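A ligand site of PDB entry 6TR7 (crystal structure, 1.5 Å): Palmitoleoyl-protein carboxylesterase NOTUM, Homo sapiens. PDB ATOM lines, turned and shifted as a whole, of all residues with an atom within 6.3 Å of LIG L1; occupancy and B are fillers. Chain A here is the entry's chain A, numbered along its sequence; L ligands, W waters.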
ATOM      1  N   GLY A  50     -10.892 -20.931 -22.059  1.00  0.00           N
ATOM      2  CA  GLY A  50     -11.521 -20.911 -23.375  1.00  0.00           C
ATOM      3  C   GLY A  50     -10.911 -19.951 -24.400  1.00  0.00           C
ATOM      4  O   GLY A  50     -11.650 -19.156 -24.993  1.00  0.00           O
ATOM      5  N   TRP A  51      -9.612 -20.026 -24.644  1.00  0.00           N
ATOM      6  CA  TRP A  51      -8.886 -19.224 -25.665  1.00  0.00           C
ATOM      7  C   TRP A  51      -9.054 -17.739 -25.350  1.00  0.00           C
ATOM      8  O   TRP A  51      -9.045 -17.365 -24.174  1.00  0.00           O
ATOM      9  CB  TRP A  51      -9.188 -19.656 -27.105  1.00  0.00           C
ATOM     10  CG  TRP A  51      -8.731 -21.081 -27.383  1.00  0.00           C
ATOM     11  CD1 TRP A  51      -9.489 -22.197 -27.301  1.00  0.00           C
ATOM     12  CD2 TRP A  51      -7.407 -21.517 -27.753  1.00  0.00           C
ATOM     13  NE1 TRP A  51      -8.746 -23.311 -27.613  1.00  0.00           N
ATOM     14  CE2 TRP A  51      -7.457 -22.912 -27.888  1.00  0.00           C
ATOM     15  CE3 TRP A  51      -6.195 -20.865 -27.988  1.00  0.00           C
ATOM     16  CZ2 TRP A  51      -6.334 -23.675 -28.244  1.00  0.00           C
ATOM     17  CZ3 TRP A  51      -5.081 -21.620 -28.351  1.00  0.00           C
ATOM     18  CH2 TRP A  51      -5.165 -23.014 -28.469  1.00  0.00           C
ATOM     19  N   TYR A  52      -9.220 -16.872 -26.370  1.00  0.00           N
ATOM     20  CA  TYR A  52      -9.235 -15.409 -26.269  1.00  0.00           C
ATOM     21  C   TYR A  52      -9.549 -14.869 -27.663  1.00  0.00           C
ATOM     22  O   TYR A  52      -9.614 -15.631 -28.629  1.00  0.00           O
ATOM     23  CB  TYR A  52      -7.909 -14.836 -25.720  1.00  0.00           C
ATOM     24  CG  TYR A  52      -6.674 -15.165 -26.548  1.00  0.00           C
ATOM     25  CD1 TYR A  52      -6.264 -14.326 -27.569  1.00  0.00           C
ATOM     26  CD2 TYR A  52      -5.935 -16.316 -26.304  1.00  0.00           C
ATOM     27  CE1 TYR A  52      -5.134 -14.611 -28.345  1.00  0.00           C
ATOM     28  CE2 TYR A  52      -4.802 -16.616 -27.074  1.00  0.00           C
ATOM     29  CZ  TYR A  52      -4.417 -15.758 -28.095  1.00  0.00           C
ATOM     30  OH  TYR A  52      -3.308 -16.039 -28.866  1.00  0.00           O
ATOM     31  N   VAL A 110      -7.634 -13.582 -21.433  1.00  0.00           N
ATOM     32  CA  VAL A 110      -6.777 -14.346 -20.524  1.00  0.00           C
ATOM     33  C   VAL A 110      -6.792 -13.745 -19.117  1.00  0.00           C
ATOM     34  O   VAL A 110      -5.795 -13.829 -18.381  1.00  0.00           O
ATOM     35  CB  VAL A 110      -5.350 -14.520 -21.098  1.00  0.00           C
ATOM     36  CG1 VAL A 110      -4.612 -15.691 -20.429  1.00  0.00           C
ATOM     37  CG2 VAL A 110      -5.408 -14.747 -22.607  1.00  0.00           C
ATOM     38  N   SER A 155      -6.532 -23.864 -18.190  1.00  0.00           N
ATOM     39  CA  SER A 155      -6.291 -23.362 -19.551  1.00  0.00           C
ATOM     40  C   SER A 155      -6.061 -21.851 -19.501  1.00  0.00           C
ATOM     41  O   SER A 155      -5.144 -21.406 -18.781  1.00  0.00           O
ATOM     42  CB  SER A 155      -7.382 -23.875 -20.480  1.00  0.00           C
ATOM     43  OG  SER A 155      -7.533 -25.291 -20.380  1.00  0.00           O
ATOM     44  N   ALA A 156      -6.829 -21.027 -20.228  1.00  0.00           N
ATOM     45  CA  ALA A 156      -6.667 -19.580 -20.084  1.00  0.00           C
ATOM     46  C   ALA A 156      -6.854 -19.153 -18.627  1.00  0.00           C
ATOM     47  O   ALA A 156      -6.243 -18.176 -18.176  1.00  0.00           O
ATOM     48  CB  ALA A 156      -7.610 -18.797 -21.013  1.00  0.00           C
ATOM     49  N   GLY A 157      -7.694 -19.887 -17.870  1.00  0.00           N
ATOM     50  CA  GLY A 157      -7.864 -19.600 -16.458  1.00  0.00           C
ATOM     51  C   GLY A 157      -6.634 -19.941 -15.627  1.00  0.00           C
ATOM     52  O   GLY A 157      -6.397 -19.322 -14.572  1.00  0.00           O
ATOM     53  N   THR A 159      -3.441 -19.625 -16.775  1.00  0.00           N
ATOM     54  CA  THR A 159      -2.607 -18.437 -16.951  1.00  0.00           C
ATOM     55  C   THR A 159      -3.178 -17.267 -16.161  1.00  0.00           C
ATOM     56  O   THR A 159      -2.416 -16.483 -15.575  1.00  0.00           O
ATOM     57  CB  THR A 159      -2.442 -18.086 -18.444  1.00  0.00           C
ATOM     58  OG1 THR A 159      -1.982 -19.234 -19.185  1.00  0.00           O
ATOM     59  CG2 THR A 159      -1.425 -16.957 -18.608  1.00  0.00           C
ATOM     60  N   GLY A 189      -2.059 -24.101 -17.896  1.00  0.00           N
ATOM     61  CA  GLY A 189      -1.801 -22.754 -18.377  1.00  0.00           C
ATOM     62  C   GLY A 189      -0.328 -22.387 -18.415  1.00  0.00           C
ATOM     63  O   GLY A 189       0.003 -21.201 -18.404  1.00  0.00           O
ATOM     64  N   PHE A 191       2.774 -22.664 -20.674  1.00  0.00           N
ATOM     65  CA  PHE A 191       3.152 -22.863 -22.069  1.00  0.00           C
ATOM     66  C   PHE A 191       4.584 -22.425 -22.365  1.00  0.00           C
ATOM     67  O   PHE A 191       5.189 -21.650 -21.613  1.00  0.00           O
ATOM     68  CB  PHE A 191       2.170 -22.113 -22.998  1.00  0.00           C
ATOM     69  CG  PHE A 191       0.746 -22.564 -22.832  1.00  0.00           C
ATOM     70  CD1 PHE A 191      -0.198 -21.727 -22.225  1.00  0.00           C
ATOM     71  CD2 PHE A 191       0.366 -23.835 -23.216  1.00  0.00           C
ATOM     72  CE1 PHE A 191      -1.509 -22.154 -22.056  1.00  0.00           C
ATOM     73  CE2 PHE A 191      -0.945 -24.262 -23.047  1.00  0.00           C
ATOM     74  CZ  PHE A 191      -1.878 -23.407 -22.449  1.00  0.00           C
ATOM     75  N   LEU A 192       5.110 -22.924 -23.480  1.00  0.00           N
ATOM     76  CA  LEU A 192       6.461 -22.605 -23.952  1.00  0.00           C
ATOM     77  C   LEU A 192       6.369 -21.760 -25.222  1.00  0.00           C
ATOM     78  O   LEU A 192       5.581 -22.069 -26.128  1.00  0.00           O
ATOM     79  CB  LEU A 192       7.249 -23.884 -24.257  1.00  0.00           C
ATOM     80  CG  LEU A 192       7.450 -24.876 -23.094  1.00  0.00           C
ATOM     81  CD1 LEU A 192       8.245 -26.076 -23.582  1.00  0.00           C
ATOM     82  CD2 LEU A 192       8.119 -24.229 -21.871  1.00  0.00           C
ATOM     83  N   PRO A 210       1.276 -17.517 -31.620  1.00  0.00           N
ATOM     84  CA  PRO A 210       0.717 -17.075 -30.333  1.00  0.00           C
ATOM     85  C   PRO A 210       1.378 -15.838 -29.732  1.00  0.00           C
ATOM     86  O   PRO A 210       0.683 -15.035 -29.100  1.00  0.00           O
ATOM     87  CB  PRO A 210       0.945 -18.309 -29.436  1.00  0.00           C
ATOM     88  CG  PRO A 210       0.847 -19.458 -30.385  1.00  0.00           C
ATOM     89  CD  PRO A 210       1.433 -18.979 -31.698  1.00  0.00           C
ATOM     90  N   THR A 211       2.698 -15.689 -29.858  1.00  0.00           N
ATOM     91  CA  THR A 211       3.336 -14.538 -29.209  1.00  0.00           C
ATOM     92  C   THR A 211       2.894 -13.234 -29.868  1.00  0.00           C
ATOM     93  O   THR A 211       2.699 -12.234 -29.172  1.00  0.00           O
ATOM     94  CB  THR A 211       4.857 -14.674 -29.230  1.00  0.00           C
ATOM     95  OG1 THR A 211       5.320 -14.841 -30.573  1.00  0.00           O
ATOM     96  CG2 THR A 211       5.296 -15.882 -28.392  1.00  0.00           C
ATOM     97  N   ILE A 214      -0.873 -12.607 -28.763  1.00  0.00           N
ATOM     98  CA  ILE A 214      -0.898 -12.060 -27.407  1.00  0.00           C
ATOM     99  C   ILE A 214      -0.399 -10.611 -27.395  1.00  0.00           C
ATOM    100  O   ILE A 214      -0.963  -9.750 -26.715  1.00  0.00           O
ATOM    101  CB  ILE A 214      -0.086 -12.958 -26.444  1.00  0.00           C
ATOM    102  CG1 ILE A 214      -0.792 -14.303 -26.235  1.00  0.00           C
ATOM    103  CG2 ILE A 214       0.132 -12.248 -25.104  1.00  0.00           C
ATOM    104  CD1 ILE A 214      -2.115 -14.182 -25.485  1.00  0.00           C
ATOM    105  N   PHE A 242       2.946 -13.684 -19.943  1.00  0.00           N
ATOM    106  CA  PHE A 242       1.912 -14.703 -20.158  1.00  0.00           C
ATOM    107  C   PHE A 242       2.486 -16.118 -20.219  1.00  0.00           C
ATOM    108  O   PHE A 242       1.709 -17.080 -20.329  1.00  0.00           O
ATOM    109  CB  PHE A 242       1.121 -14.399 -21.442  1.00  0.00           C
ATOM    110  CG  PHE A 242       0.106 -13.288 -21.315  1.00  0.00           C
ATOM    111  CD1 PHE A 242       0.497 -11.997 -21.012  1.00  0.00           C
ATOM    112  CD2 PHE A 242      -1.241 -13.538 -21.539  1.00  0.00           C
ATOM    113  CE1 PHE A 242      -0.430 -10.955 -20.896  1.00  0.00           C
ATOM    114  CE2 PHE A 242      -2.171 -12.494 -21.433  1.00  0.00           C
ATOM    115  CZ  PHE A 242      -1.768 -11.213 -21.113  1.00  0.00           C
ATOM    116  N   PHE A 243       3.823 -16.264 -20.141  1.00  0.00           N
ATOM    117  CA  PHE A 243       4.486 -17.558 -20.183  1.00  0.00           C
ATOM    118  C   PHE A 243       4.933 -17.938 -18.771  1.00  0.00           C
ATOM    119  O   PHE A 243       5.751 -17.226 -18.171  1.00  0.00           O
ATOM    120  CB  PHE A 243       5.623 -17.515 -21.203  1.00  0.00           C
ATOM    121  CG  PHE A 243       5.102 -17.513 -22.619  1.00  0.00           C
ATOM    122  CD1 PHE A 243       4.706 -16.326 -23.230  1.00  0.00           C
ATOM    123  CD2 PHE A 243       4.901 -18.709 -23.285  1.00  0.00           C
ATOM    124  CE1 PHE A 243       4.144 -16.336 -24.514  1.00  0.00           C
ATOM    125  CE2 PHE A 243       4.368 -18.729 -24.578  1.00  0.00           C
ATOM    126  CZ  PHE A 243       3.988 -17.542 -25.182  1.00  0.00           C
ATOM    127  N   ASP A 263       0.953 -31.304 -23.694  1.00  0.00           N
ATOM    128  CA  ASP A 263      -0.366 -30.675 -23.680  1.00  0.00           C
ATOM    129  C   ASP A 263      -0.894 -30.461 -25.101  1.00  0.00           C
ATOM    130  O   ASP A 263      -0.171 -30.023 -26.002  1.00  0.00           O
ATOM    131  CB  ASP A 263      -0.242 -29.358 -22.909  1.00  0.00           C
ATOM    132  CG  ASP A 263      -1.526 -28.592 -22.842  1.00  0.00           C
ATOM    133  OD1 ASP A 263      -2.289 -28.819 -21.888  1.00  0.00           O
ATOM    134  OD2 ASP A 263      -1.779 -27.790 -23.744  1.00  0.00           O
ATOM    135  N   ALA A 265      -3.061 -28.285 -26.341  1.00  0.00           N
ATOM    136  CA  ALA A 265      -3.087 -26.913 -26.853  1.00  0.00           C
ATOM    137  C   ALA A 265      -1.687 -26.455 -27.273  1.00  0.00           C
ATOM    138  O   ALA A 265      -1.533 -25.770 -28.295  1.00  0.00           O
ATOM    139  CB  ALA A 265      -3.701 -25.964 -25.820  1.00  0.00           C
ATOM    140  N   GLN A 266      -0.665 -26.831 -26.492  1.00  0.00           N
ATOM    141  CA  GLN A 266       0.723 -26.547 -26.864  1.00  0.00           C
ATOM    142  C   GLN A 266       1.049 -27.169 -28.215  1.00  0.00           C
ATOM    143  O   GLN A 266       1.615 -26.503 -29.096  1.00  0.00           O
ATOM    144  CB  GLN A 266       1.663 -27.090 -25.777  1.00  0.00           C
ATOM    145  CG  GLN A 266       3.147 -26.924 -26.102  1.00  0.00           C
ATOM    146  CD  GLN A 266       3.660 -25.513 -25.798  1.00  0.00           C
ATOM    147  OE1 GLN A 266       3.485 -25.000 -24.700  1.00  0.00           O
ATOM    148  NE2 GLN A 266       4.299 -24.899 -26.799  1.00  0.00           N
ATOM    149  N   VAL A 269      -0.688 -25.266 -31.263  1.00  0.00           N
ATOM    150  CA  VAL A 269      -0.048 -24.026 -31.670  1.00  0.00           C
ATOM    151  C   VAL A 269       1.366 -24.244 -32.188  1.00  0.00           C
ATOM    152  O   VAL A 269       1.900 -23.393 -32.908  1.00  0.00           O
ATOM    153  CB  VAL A 269      -0.176 -22.919 -30.600  1.00  0.00           C
ATOM    154  CG1 VAL A 269      -1.643 -22.742 -30.205  1.00  0.00           C
ATOM    155  CG2 VAL A 269       0.693 -23.219 -29.362  1.00  0.00           C
HETATM  156  N1  LIG L   1      -0.004 -20.809 -25.772  1.00  0.00           N
HETATM  157  C1  LIG L   1       0.270 -18.335 -25.616  1.00  0.00           C
HETATM  158  C2  LIG L   1      -0.412 -18.337 -24.285  1.00  0.00           C
HETATM  159  C3  LIG L   1       0.151 -18.093 -23.065  1.00  0.00           C
HETATM  160  C4  LIG L   1      -1.994 -18.565 -22.649  1.00  0.00           C
HETATM  161  C5  LIG L   1      -1.791 -18.648 -24.046  1.00  0.00           C
HETATM  162  C6  LIG L   1      -4.070 -19.225 -24.293  1.00  0.00           C
HETATM  163  C7  LIG L   1      -1.779 -22.346 -26.301  1.00  0.00           C
HETATM  164  C8  LIG L   1      -4.283 -19.145 -22.916  1.00  0.00           C
HETATM  165  C9  LIG L   1      -3.236 -18.810 -22.080  1.00  0.00           C
HETATM  166  C10 LIG L   1      -0.978 -21.125 -26.631  1.00  0.00           C
HETATM  167  C11 LIG L   1       0.891 -19.682 -25.975  1.00  0.00           C
HETATM  168  C12 LIG L   1      -2.858 -18.992 -24.881  1.00  0.00           C
HETATM  169  F1  LIG L   1      -5.128 -19.565 -25.077  1.00  0.00           F
HETATM  170  N2  LIG L   1      -0.793 -18.226 -22.084  1.00  0.00           N
HETATM  171  O1  LIG L   1      -1.201 -20.457 -27.630  1.00  0.00           O
HETATM  172  N1  LG2 L   2       6.172 -20.214 -30.411  1.00  0.00           N
HETATM  173  C1  LG2 L   2       7.776 -18.311 -30.571  1.00  0.00           C
HETATM  174  C2  LG2 L   2       8.667 -17.595 -31.540  1.00  0.00           C
HETATM  175  C3  LG2 L   2       8.401 -16.457 -32.230  1.00  0.00           C
HETATM  176  C4  LG2 L   2      10.445 -17.076 -32.882  1.00  0.00           C
HETATM  177  C5  LG2 L   2       9.984 -18.023 -31.948  1.00  0.00           C
HETATM  178  C6  LG2 L   2      12.029 -19.191 -32.186  1.00  0.00           C
HETATM  179  C7  LG2 L   2       4.273 -21.153 -29.250  1.00  0.00           C
HETATM  180  C8  LG2 L   2      12.495 -18.273 -33.118  1.00  0.00           C
HETATM  181  C9  LG2 L   2      11.703 -17.203 -33.474  1.00  0.00           C
HETATM  182  C10 LG2 L   2       4.936 -19.995 -29.951  1.00  0.00           C
HETATM  183  C11 LG2 L   2       6.848 -19.276 -31.287  1.00  0.00           C
HETATM  184  C12 LG2 L   2      10.798 -19.099 -31.588  1.00  0.00           C
HETATM  185  F1  LG2 L   2      12.844 -20.241 -31.842  1.00  0.00           F
HETATM  186  N2  LG2 L   2       9.461 -16.143 -33.040  1.00  0.00           N
HETATM  187  O1  LG2 L   2       4.375 -18.903 -30.098  1.00  0.00           O
HETATM  188  O   HOH W   1      -3.049 -18.656 -29.143  1.00  0.00           O
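Merely in contact with LIG L1: Trp 51, Tyr 52, Val 110, Ala 156, Phe 191, Pro 210, Phe 243, Ala 265 and Val 269. Hydrophobic or aromatic side chains that line LIG L1: Trp 51, Tyr 52, Val 110, Ala 156, Phe 191, Pro 210, Phe 243 and Val 269. Along chain A the residues within 4 Å of LIG L1 span positions 51 to 269.
The backbone carbonyl oxygen (O) of Phe 242 is in hydrogen-bond range of a nitrogen (N2) of LIG L1, at 3.3 Å. N2 of LIG L1 lies close to OG1 of Thr 159 (3.3 Å).
Water W1 bridges the side-chain hydroxyl (OH) of Tyr 52 (2.6 Å) and an oxygen (O1) of LIG L1 (3.0 Å).
N of Ala 265 sits at hydrogen-bond distance from OD2 of Asp 263. The backbone carbonyl oxygen (O) of Gly 189 sits at hydrogen-bond distance from the side-chain hydroxyl (OG1) of Thr 159 (2.9 Å).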
